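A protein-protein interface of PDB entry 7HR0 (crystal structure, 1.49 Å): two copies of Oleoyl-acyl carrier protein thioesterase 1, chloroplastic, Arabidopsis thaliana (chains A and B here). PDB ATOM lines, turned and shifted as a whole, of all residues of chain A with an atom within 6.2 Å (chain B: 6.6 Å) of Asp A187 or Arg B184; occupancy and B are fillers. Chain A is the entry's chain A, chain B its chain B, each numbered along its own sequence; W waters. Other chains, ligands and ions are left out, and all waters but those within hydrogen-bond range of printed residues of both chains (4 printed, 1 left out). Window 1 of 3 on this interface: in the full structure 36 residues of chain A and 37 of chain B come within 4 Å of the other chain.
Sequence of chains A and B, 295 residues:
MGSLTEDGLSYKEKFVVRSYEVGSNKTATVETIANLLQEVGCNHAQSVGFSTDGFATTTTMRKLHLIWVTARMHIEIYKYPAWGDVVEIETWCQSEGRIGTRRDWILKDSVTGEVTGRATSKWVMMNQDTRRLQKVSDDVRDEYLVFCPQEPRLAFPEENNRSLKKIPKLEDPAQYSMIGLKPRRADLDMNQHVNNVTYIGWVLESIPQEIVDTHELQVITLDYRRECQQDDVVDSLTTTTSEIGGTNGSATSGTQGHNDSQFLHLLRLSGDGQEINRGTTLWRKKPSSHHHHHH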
ATOM      1  N   GLU A  31      -1.980  -8.036  23.456  1.00  0.00           N
ATOM      2  CA  GLU A  31      -1.541  -6.627  23.506  1.00  0.00           C
ATOM      3  C   GLU A  31      -2.198  -5.798  22.377  1.00  0.00           C
ATOM      4  O   GLU A  31      -2.594  -4.637  22.616  1.00  0.00           O
ATOM      5  CB  GLU A  31      -0.023  -6.522  23.432  1.00  0.00           C
ATOM      6  CG  GLU A  31       0.571  -7.094  24.695  1.00  0.00           C
ATOM      7  CD  GLU A  31       2.070  -6.991  24.676  1.00  0.00           C
ATOM      8  OE1 GLU A  31       2.723  -8.026  24.402  1.00  0.00           O
ATOM      9  OE2 GLU A  31       2.584  -5.886  24.981  1.00  0.00           O
ATOM     10  N   LEU A 181      13.883  -6.233  32.242  1.00  0.00           N
ATOM     11  CA  LEU A 181      12.995  -5.601  31.250  1.00  0.00           C
ATOM     12  C   LEU A 181      12.991  -4.096  31.427  1.00  0.00           C
ATOM     13  O   LEU A 181      12.987  -3.616  32.558  1.00  0.00           O
ATOM     14  CB  LEU A 181      11.589  -6.132  31.442  1.00  0.00           C
ATOM     15  CG  LEU A 181      11.486  -7.637  31.138  1.00  0.00           C
ATOM     16  CD1 LEU A 181      10.136  -8.212  31.666  1.00  0.00           C
ATOM     17  CD2 LEU A 181      11.600  -7.890  29.607  1.00  0.00           C
ATOM     18  N   LYS A 182      13.059  -3.345  30.323  1.00  0.00           N
ATOM     19  CA  LYS A 182      13.045  -1.893  30.438  1.00  0.00           C
ATOM     20  C   LYS A 182      12.308  -1.266  29.275  1.00  0.00           C
ATOM     21  O   LYS A 182      12.345  -1.791  28.150  1.00  0.00           O
ATOM     22  CB  LYS A 182      14.429  -1.289  30.627  1.00  0.00           C
ATOM     23  CG  LYS A 182      15.362  -1.354  29.460  1.00  0.00           C
ATOM     24  CD  LYS A 182      16.803  -0.998  29.932  1.00  0.00           C
ATOM     25  CE  LYS A 182      17.820  -1.147  28.814  1.00  0.00           C
ATOM     26  NZ  LYS A 182      19.207  -0.777  29.236  1.00  0.00           N
ATOM     27  N   PRO A 183      11.596  -0.163  29.555  1.00  0.00           N
ATOM     28  CA  PRO A 183      10.822   0.470  28.489  1.00  0.00           C
ATOM     29  C   PRO A 183      11.697   1.252  27.517  1.00  0.00           C
ATOM     30  O   PRO A 183      12.731   1.832  27.912  1.00  0.00           O
ATOM     31  CB  PRO A 183       9.870   1.429  29.256  1.00  0.00           C
ATOM     32  CG  PRO A 183      10.630   1.798  30.508  1.00  0.00           C
ATOM     33  CD  PRO A 183      11.415   0.525  30.867  1.00  0.00           C
ATOM     34  N   ARG A 184      11.318   1.219  26.247  1.00  0.00           N
ATOM     35  CA  ARG A 184      11.984   2.055  25.251  1.00  0.00           C
ATOM     36  C   ARG A 184      10.954   3.182  24.904  1.00  0.00           C
ATOM     37  O   ARG A 184       9.820   3.157  25.429  1.00  0.00           O
ATOM     38  CB  ARG A 184      12.498   1.252  24.042  1.00  0.00           C
ATOM     39  CG  ARG A 184      11.467   0.431  23.282  1.00  0.00           C
ATOM     40  CD  ARG A 184      12.180  -0.461  22.244  1.00  0.00           C
ATOM     41  NE  ARG A 184      11.290  -1.329  21.463  1.00  0.00           N
ATOM     42  CZ  ARG A 184      10.693  -0.965  20.323  1.00  0.00           C
ATOM     43  NH1 ARG A 184      10.816   0.281  19.866  1.00  0.00           N
ATOM     44  NH2 ARG A 184       9.933  -1.829  19.659  1.00  0.00           N
ATOM     45  N   ARG A 185      11.318   4.160  24.057  1.00  0.00           N
ATOM     46  CA  ARG A 185      10.406   5.300  23.810  1.00  0.00           C
ATOM     47  C   ARG A 185       9.064   4.900  23.283  1.00  0.00           C
ATOM     48  O   ARG A 185       8.053   5.533  23.608  1.00  0.00           O
ATOM     49  CB  ARG A 185      11.031   6.363  22.884  1.00  0.00           C
ATOM     50  CG  ARG A 185      12.234   7.030  23.529  1.00  0.00           C
ATOM     51  CD  ARG A 185      12.421   8.456  23.012  1.00  0.00           C
ATOM     52  NE  ARG A 185      13.675   8.973  23.536  1.00  0.00           N
ATOM     53  CZ  ARG A 185      14.844   8.878  22.909  1.00  0.00           C
ATOM     54  NH1 ARG A 185      14.911   8.368  21.682  1.00  0.00           N
ATOM     55  NH2 ARG A 185      15.944   9.335  23.484  1.00  0.00           N
ATOM     56  N   ALA A 186       9.028   3.839  22.451  1.00  0.00           N
ATOM     57  CA  ALA A 186       7.749   3.382  21.863  1.00  0.00           C
ATOM     58  C   ALA A 186       6.774   2.890  22.972  1.00  0.00           C
ATOM     59  O   ALA A 186       5.572   2.798  22.745  1.00  0.00           O
ATOM     60  CB  ALA A 186       8.013   2.265  20.864  1.00  0.00           C
ATOM     61  N   ASP A 187       7.310   2.494  24.151  1.00  0.00           N
ATOM     62  CA  ASP A 187       6.469   2.063  25.276  1.00  0.00           C
ATOM     63  C   ASP A 187       5.858   3.228  26.043  1.00  0.00           C
ATOM     64  O   ASP A 187       5.087   2.966  26.969  1.00  0.00           O
ATOM     65  CB  ASP A 187       7.309   1.265  26.282  1.00  0.00           C
ATOM     66  CG  ASP A 187       7.755  -0.055  25.691  1.00  0.00           C
ATOM     67  OD1 ASP A 187       6.868  -0.817  25.189  1.00  0.00           O
ATOM     68  OD2 ASP A 187       8.980  -0.345  25.732  1.00  0.00           O
ATOM     69  N   LEU A 188       6.251   4.462  25.742  1.00  0.00           N
ATOM     70  CA  LEU A 188       5.721   5.607  26.473  1.00  0.00           C
ATOM     71  C   LEU A 188       4.531   6.204  25.742  1.00  0.00           C
ATOM     72  O   LEU A 188       4.411   6.079  24.514  1.00  0.00           O
ATOM     73  CB  LEU A 188       6.807   6.672  26.702  1.00  0.00           C
ATOM     74  CG  LEU A 188       8.111   6.143  27.344  1.00  0.00           C
ATOM     75  CD1 LEU A 188       9.203   7.225  27.447  1.00  0.00           C
ATOM     76  CD2 LEU A 188       7.851   5.421  28.677  1.00  0.00           C
ATOM     77  N   ASP A 189       3.641   6.864  26.507  1.00  0.00           N
ATOM     78  CA  ASP A 189       2.497   7.571  25.938  1.00  0.00           C
ATOM     79  C   ASP A 189       2.878   9.023  25.596  1.00  0.00           C
ATOM     80  O   ASP A 189       4.027   9.425  25.767  1.00  0.00           O
ATOM     81  CB  ASP A 189       1.258   7.458  26.857  1.00  0.00           C
ATOM     82  CG  ASP A 189       1.377   8.105  28.226  1.00  0.00           C
ATOM     83  OD1 ASP A 189       2.316   8.901  28.435  1.00  0.00           O
ATOM     84  OD2 ASP A 189       0.542   7.792  29.104  1.00  0.00           O
ATOM     85  N   HIS A 193       4.681   8.746  30.098  1.00  0.00           N
ATOM     86  CA  HIS A 193       4.429   7.704  31.104  1.00  0.00           C
ATOM     87  C   HIS A 193       4.422   6.339  30.385  1.00  0.00           C
ATOM     88  O   HIS A 193       4.000   6.269  29.231  1.00  0.00           O
ATOM     89  CB  HIS A 193       3.064   7.900  31.785  1.00  0.00           C
ATOM     90  CG  HIS A 193       3.037   9.024  32.788  1.00  0.00           C
ATOM     91  ND1 HIS A 193       2.935   8.775  34.143  1.00  0.00           N
ATOM     92  CD2 HIS A 193       3.086  10.363  32.594  1.00  0.00           C
ATOM     93  CE1 HIS A 193       2.955   9.967  34.737  1.00  0.00           C
ATOM     94  NE2 HIS A 193       3.047  10.954  33.844  1.00  0.00           N
ATOM     95  N   VAL A 194       4.820   5.238  31.075  1.00  0.00           N
ATOM     96  CA  VAL A 194       4.764   3.916  30.417  1.00  0.00           C
ATOM     97  C   VAL A 194       3.294   3.574  30.100  1.00  0.00           C
ATOM     98  O   VAL A 194       2.412   3.778  30.956  1.00  0.00           O
ATOM     99  CB  VAL A 194       5.452   2.829  31.284  1.00  0.00           C
ATOM    100  CG1 VAL A 194       5.276   1.445  30.673  1.00  0.00           C
ATOM    101  CG2 VAL A 194       6.925   3.158  31.475  1.00  0.00           C
ATOM    102  N   ASN A 195       3.029   3.135  28.863  1.00  0.00           N
ATOM    103  CA  ASN A 195       1.666   2.799  28.447  1.00  0.00           C
ATOM    104  C   ASN A 195       1.172   1.602  29.244  1.00  0.00           C
ATOM    105  O   ASN A 195       1.937   0.644  29.457  1.00  0.00           O
ATOM    106  CB  ASN A 195       1.654   2.474  26.942  1.00  0.00           C
ATOM    107  CG  ASN A 195       0.243   2.392  26.399  1.00  0.00           C
ATOM    108  OD1 ASN A 195      -0.538   1.525  26.797  1.00  0.00           O
ATOM    109  ND2 ASN A 195      -0.147   3.338  25.538  1.00  0.00           N
ATOM    110  N   ASN A 196      -0.099   1.618  29.664  1.00  0.00           N
ATOM    111  CA  ASN A 196      -0.662   0.507  30.424  1.00  0.00           C
ATOM    112  C   ASN A 196      -0.493  -0.847  29.730  1.00  0.00           C
ATOM    113  O   ASN A 196      -0.411  -1.876  30.404  1.00  0.00           O
ATOM    114  CB  ASN A 196      -2.165   0.722  30.622  1.00  0.00           C
ATOM    115  CG  ASN A 196      -2.516   1.692  31.695  1.00  0.00           C
ATOM    116  OD1 ASN A 196      -1.683   2.023  32.573  1.00  0.00           O
ATOM    117  ND2 ASN A 196      -3.791   2.163  31.656  1.00  0.00           N
ATOM    118  N   VAL A 197      -0.553  -0.857  28.376  1.00  0.00           N
ATOM    119  CA  VAL A 197      -0.466  -2.128  27.654  1.00  0.00           C
ATOM    120  C   VAL A 197       0.949  -2.761  27.809  1.00  0.00           C
ATOM    121  O   VAL A 197       1.090  -3.994  27.757  1.00  0.00           O
ATOM    122  CB  VAL A 197      -0.797  -1.932  26.166  1.00  0.00           C
ATOM    123  CG1 VAL A 197      -0.665  -3.244  25.424  1.00  0.00           C
ATOM    124  CG2 VAL A 197      -2.203  -1.330  26.005  1.00  0.00           C
ATOM    125  N   THR A 198       1.993  -1.919  28.000  1.00  0.00           N
ATOM    126  CA  THR A 198       3.356  -2.447  28.119  1.00  0.00           C
ATOM    127  C   THR A 198       3.482  -3.427  29.283  1.00  0.00           C
ATOM    128  O   THR A 198       4.160  -4.460  29.159  1.00  0.00           O
ATOM    129  CB  THR A 198       4.365  -1.277  28.276  1.00  0.00           C
ATOM    130  OG1 THR A 198       4.316  -0.507  27.061  1.00  0.00           O
ATOM    131  CG2 THR A 198       5.794  -1.789  28.485  1.00  0.00           C
ATOM    132  N   ILE A 200       1.208  -5.456  30.451  1.00  0.00           N
ATOM    133  CA  ILE A 200       0.663  -6.763  30.045  1.00  0.00           C
ATOM    134  C   ILE A 200       1.783  -7.574  29.312  1.00  0.00           C
ATOM    135  O   ILE A 200       2.045  -8.738  29.626  1.00  0.00           O
ATOM    136  CB  ILE A 200      -0.541  -6.567  29.104  1.00  0.00           C
ATOM    137  CG1 ILE A 200      -1.683  -5.967  29.894  1.00  0.00           C
ATOM    138  CG2 ILE A 200      -0.924  -7.921  28.460  1.00  0.00           C
ATOM    139  CD1 ILE A 200      -2.972  -5.661  29.066  1.00  0.00           C
ATOM    140  N   GLY A 201       2.472  -6.920  28.370  1.00  0.00           N
ATOM    141  CA  GLY A 201       3.579  -7.565  27.661  1.00  0.00           C
ATOM    142  C   GLY A 201       4.656  -8.057  28.614  1.00  0.00           C
ATOM    143  O   GLY A 201       5.125  -9.203  28.507  1.00  0.00           O
ATOM    144  N   TRP A 202       4.992  -7.207  29.609  1.00  0.00           N
ATOM    145  CA  TRP A 202       6.017  -7.633  30.596  1.00  0.00           C
ATOM    146  C   TRP A 202       5.557  -8.813  31.435  1.00  0.00           C
ATOM    147  O   TRP A 202       6.353  -9.724  31.751  1.00  0.00           O
ATOM    148  CB  TRP A 202       6.441  -6.459  31.467  1.00  0.00           C
ATOM    149  CG  TRP A 202       7.273  -5.423  30.771  1.00  0.00           C
ATOM    150  CD1 TRP A 202       8.048  -5.576  29.651  1.00  0.00           C
ATOM    151  CD2 TRP A 202       7.434  -4.067  31.192  1.00  0.00           C
ATOM    152  NE1 TRP A 202       8.703  -4.390  29.366  1.00  0.00           N
ATOM    153  CE2 TRP A 202       8.345  -3.451  30.303  1.00  0.00           C
ATOM    154  CE3 TRP A 202       6.869  -3.308  32.220  1.00  0.00           C
ATOM    155  CZ2 TRP A 202       8.731  -2.116  30.442  1.00  0.00           C
ATOM    156  CZ3 TRP A 202       7.186  -1.955  32.306  1.00  0.00           C
ATOM    157  CH2 TRP A 202       8.138  -1.383  31.448  1.00  0.00           C
ATOM    158  N   GLU A 205       5.948 -12.003  29.425  1.00  0.00           N
ATOM    159  CA  GLU A 205       7.302 -12.415  29.073  1.00  0.00           C
ATOM    160  C   GLU A 205       7.810 -13.631  29.848  1.00  0.00           C
ATOM    161  O   GLU A 205       8.694 -14.336  29.349  1.00  0.00           O
ATOM    162  CB  GLU A 205       8.303 -11.266  29.271  1.00  0.00           C
ATOM    163  CG  GLU A 205       8.519 -10.392  28.047  1.00  0.00           C
ATOM    164  CD  GLU A 205       8.854 -11.119  26.745  1.00  0.00           C
ATOM    165  OE1 GLU A 205       7.916 -11.344  25.955  1.00  0.00           O
ATOM    166  OE2 GLU A 205      10.048 -11.387  26.477  1.00  0.00           O
ATOM    167  N   LYS B 182      16.634  -5.819  24.439  1.00  0.00           N
ATOM    168  CA  LYS B 182      16.237  -7.149  24.010  1.00  0.00           C
ATOM    169  C   LYS B 182      14.791  -7.166  23.583  1.00  0.00           C
ATOM    170  O   LYS B 182      13.969  -6.426  24.134  1.00  0.00           O
ATOM    171  CB  LYS B 182      16.545  -8.223  25.047  1.00  0.00           C
ATOM    172  CG  LYS B 182      15.744  -8.197  26.310  1.00  0.00           C
ATOM    173  CD  LYS B 182      16.384  -9.159  27.355  1.00  0.00           C
ATOM    174  CE  LYS B 182      15.701  -9.092  28.706  1.00  0.00           C
ATOM    175  NZ  LYS B 182      16.318 -10.024  29.712  1.00  0.00           N
ATOM    176  N   PRO B 183      14.481  -7.988  22.570  1.00  0.00           N
ATOM    177  CA  PRO B 183      13.101  -8.018  22.080  1.00  0.00           C
ATOM    178  C   PRO B 183      12.164  -8.799  23.003  1.00  0.00           C
ATOM    179  O   PRO B 183      12.585  -9.773  23.670  1.00  0.00           O
ATOM    180  CB  PRO B 183      13.225  -8.730  20.710  1.00  0.00           C
ATOM    181  CG  PRO B 183      14.416  -9.659  20.869  1.00  0.00           C
ATOM    182  CD  PRO B 183      15.380  -8.865  21.771  1.00  0.00           C
ATOM    183  N   ARG B 184      10.944  -8.312  23.123  1.00  0.00           N
ATOM    184  CA  ARG B 184       9.919  -9.045  23.852  1.00  0.00           C
ATOM    185  C   ARG B 184       8.952  -9.611  22.748  1.00  0.00           C
ATOM    186  O   ARG B 184       9.150  -9.312  21.553  1.00  0.00           O
ATOM    187  CB  ARG B 184       9.226  -8.194  24.939  1.00  0.00           C
ATOM    188  CG  ARG B 184       8.579  -6.891  24.468  1.00  0.00           C
ATOM    189  CD  ARG B 184       8.131  -6.075  25.697  1.00  0.00           C
ATOM    190  NE  ARG B 184       7.514  -4.785  25.379  1.00  0.00           N
ATOM    191  CZ  ARG B 184       6.208  -4.621  25.142  1.00  0.00           C
ATOM    192  NH1 ARG B 184       5.394  -5.678  25.095  1.00  0.00           N
ATOM    193  NH2 ARG B 184       5.715  -3.405  24.896  1.00  0.00           N
ATOM    194  N   ARG B 185       7.929 -10.398  23.122  1.00  0.00           N
ATOM    195  CA  ARG B 185       7.086 -11.041  22.098  1.00  0.00           C
ATOM    196  C   ARG B 185       6.416 -10.085  21.169  1.00  0.00           C
ATOM    197  O   ARG B 185       6.237 -10.395  19.983  1.00  0.00           O
ATOM    198  CB  ARG B 185       6.039 -11.991  22.714  1.00  0.00           C
ATOM    199  CG  ARG B 185       6.704 -13.174  23.416  1.00  0.00           C
ATOM    200  CD  ARG B 185       5.808 -14.404  23.392  1.00  0.00           C
ATOM    201  NE  ARG B 185       6.389 -15.409  24.260  1.00  0.00           N
ATOM    202  CZ  ARG B 185       6.063 -15.572  25.536  1.00  0.00           C
ATOM    203  NH1 ARG B 185       5.084 -14.851  26.078  1.00  0.00           N
ATOM    204  NH2 ARG B 185       6.680 -16.486  26.266  1.00  0.00           N
ATOM    205  N   ALA B 186       6.019  -8.905  21.684  1.00  0.00           N
ATOM    206  CA  ALA B 186       5.334  -7.899  20.852  1.00  0.00           C
ATOM    207  C   ALA B 186       6.266  -7.400  19.713  1.00  0.00           C
ATOM    208  O   ALA B 186       5.794  -6.847  18.732  1.00  0.00           O
ATOM    209  CB  ALA B 186       4.898  -6.722  21.721  1.00  0.00           C
ATOM    210  N   ASP B 187       7.609  -7.528  19.891  1.00  0.00           N
ATOM    211  CA  ASP B 187       8.566  -7.122  18.848  1.00  0.00           C
ATOM    212  C   ASP B 187       8.701  -8.152  17.737  1.00  0.00           C
ATOM    213  O   ASP B 187       9.441  -7.881  16.786  1.00  0.00           O
ATOM    214  CB  ASP B 187       9.963  -6.953  19.467  1.00  0.00           C
ATOM    215  CG  ASP B 187       9.998  -5.767  20.410  1.00  0.00           C
ATOM    216  OD1 ASP B 187       9.604  -4.644  19.973  1.00  0.00           O
ATOM    217  OD2 ASP B 187      10.434  -5.941  21.581  1.00  0.00           O
ATOM    218  N   LEU B 188       8.100  -9.327  17.888  1.00  0.00           N
ATOM    219  CA  LEU B 188       8.229 -10.360  16.864  1.00  0.00           C
ATOM    220  C   LEU B 188       7.071 -10.293  15.890  1.00  0.00           C
ATOM    221  O   LEU B 188       5.977  -9.845  16.250  1.00  0.00           O
ATOM    222  CB  LEU B 188       8.324 -11.762  17.500  1.00  0.00           C
ATOM    223  CG  LEU B 188       9.415 -11.901  18.592  1.00  0.00           C
ATOM    224  CD1 LEU B 188       9.416 -13.282  19.283  1.00  0.00           C
ATOM    225  CD2 LEU B 188      10.809 -11.501  18.082  1.00  0.00           C
ATOM    226  N   TRP B 202      15.356   0.662  18.367  1.00  0.00           N
ATOM    227  CA  TRP B 202      16.646   0.446  19.058  1.00  0.00           C
ATOM    228  C   TRP B 202      17.705   1.460  18.650  1.00  0.00           C
ATOM    229  O   TRP B 202      18.510   1.920  19.483  1.00  0.00           O
ATOM    230  CB  TRP B 202      17.137  -0.987  18.849  1.00  0.00           C
ATOM    231  CG  TRP B 202      16.345  -2.030  19.581  1.00  0.00           C
ATOM    232  CD1 TRP B 202      15.577  -1.875  20.703  1.00  0.00           C
ATOM    233  CD2 TRP B 202      16.290  -3.417  19.240  1.00  0.00           C
ATOM    234  NE1 TRP B 202      15.058  -3.100  21.092  1.00  0.00           N
ATOM    235  CE2 TRP B 202      15.494  -4.063  20.214  1.00  0.00           C
ATOM    236  CE3 TRP B 202      16.811  -4.168  18.183  1.00  0.00           C
ATOM    237  CZ2 TRP B 202      15.240  -5.436  20.170  1.00  0.00           C
ATOM    238  CZ3 TRP B 202      16.493  -5.516  18.097  1.00  0.00           C
ATOM    239  CH2 TRP B 202      15.748  -6.143  19.106  1.00  0.00           C
ATOM    240  N   GLN B 230      15.577 -13.929  18.581  1.00  0.00           N
ATOM    241  CA  GLN B 230      14.710 -13.617  19.728  1.00  0.00           C
ATOM    242  C   GLN B 230      15.414 -13.769  21.083  1.00  0.00           C
ATOM    243  O   GLN B 230      14.978 -13.147  22.054  1.00  0.00           O
ATOM    244  CB  GLN B 230      13.384 -14.394  19.666  1.00  0.00           C
ATOM    245  CG  GLN B 230      13.444 -15.825  20.128  1.00  0.00           C
ATOM    246  CD  GLN B 230      12.005 -16.293  20.226  1.00  0.00           C
ATOM    247  OE1 GLN B 230      11.260 -15.911  21.148  1.00  0.00           O
ATOM    248  NE2 GLN B 230      11.570 -17.088  19.253  1.00  0.00           N
HETATM  249  O   HOH W   1      12.393  -9.644  26.713  1.00  0.00           O
HETATM  250  O   HOH W   2       9.593  -2.913  25.107  1.00  0.00           O
HETATM  251  O   HOH W   3       2.973  -3.400  24.078  1.00  0.00           O
HETATM  252  O   HOH W   4      10.891  -3.655  22.939  1.00  0.00           O
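Water W3 bridges OE2 of Glu A31 (2.7 Å) and NH2 of Arg B184 (2.9 Å). Water W4 bridges the side-chain carboxylate of Asp B187 (2.7 Å) and the guanidinium group of Arg A184 (2.8 Å). Water W2 bridges OD2 of Asp A187 (2.7 Å) and NE of Arg B184 (2.8 Å). Water W1 bridges the side-chain carboxylate (OE2) of Glu A205 (2.9 Å) and the backbone carbonyl oxygen (O) of Pro B183 (3.1 Å).
Among the printed residues, pairs that only touch across the chains: Glu A205 with Arg B184 (3.5 Å), Gly A201 with Arg B184 (3.7 Å), Glu A31 with Ala B186 (3.7 Å), Thr A198 with Arg B184 (3.9 Å), Trp A202 with Arg B184 (3.99 Å) and Arg A184 with Trp B202 (3.99 Å).
OD2 of Asp A187 lies within hydrogen-bond range of N of Arg A184, 2.9 Å away. N of Asn A195 sits at hydrogen-bond distance from O of Asp A187 (2.8 Å). The side-chain hydroxyl of Thr A198 lies within hydrogen-bond range of the side-chain carboxylate of Asp A187, 3.2 Å away. The backbone NH of Arg B184 is in hydrogen-bond range of the side-chain carboxylate of Asp B187.
Of the 20 printed residues of chain A, 7 touch a printed residue of chain B. Hydrophobic or aromatic side chains of chain A that line the printed part of chain B: Trp A202. Of the 9 printed residues of chain B, 5 touch a printed residue of chain A. Among the printed residues, 10 pairs touch across the chains.
Lys A182 touches none of the printed residues of chain B. Of chain B, only Arg B184 (2.8 Å) comes within 4 Å of Asp A187. Of the printed residues of chain B, Thr A198 touches Arg B184. Of the printed residues of chain B, Gly A201 touches Arg B184. Of the printed residues of chain B, Trp A202 touches Arg B184 (3.99 Å). Of the printed residues of chain B, Glu A205 touches Arg B184 (3.5 Å) and Arg B185 (3.0 Å). Pro B183 touches none of the printed residues of chain A. Printed residues of chain A within 4 Å of Arg B184: Glu A31 (2.8 Å), Asp A187 (2.8 Å), Thr A198 (3.9 Å), Gly A201 (3.7 Å), Trp A202 (3.99 Å) and Glu A205 (3.5 Å). Of the printed residues of chain A, Arg B185 touches Glu A205. The nearest printed residue of chain B that does not touch Asp A187 is Asp B187 (7.0 Å).
Arg A184 touches Asp B187, and with the chains exchanged Asp A187 touches Arg B184. Arg A184 touches Trp B202, and with the chains exchanged Trp A202 touches Arg B184.
The side-chain carboxylate of Glu A31 lies within salt-bridge range of the guanidinium group of Arg B184. The side-chain carboxylate of Asp B187 is in salt-bridge range of the guanidinium group of Arg A184, at 2.9 Å. OD1 of Asp A187 lies within salt-bridge range of NH2 of Arg B184 (2.8 Å). The side-chain carboxylate (OE1) of Glu A205 sits at hydrogen-bond distance from the backbone NH (N) of Arg B185, 3.0 Å away.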
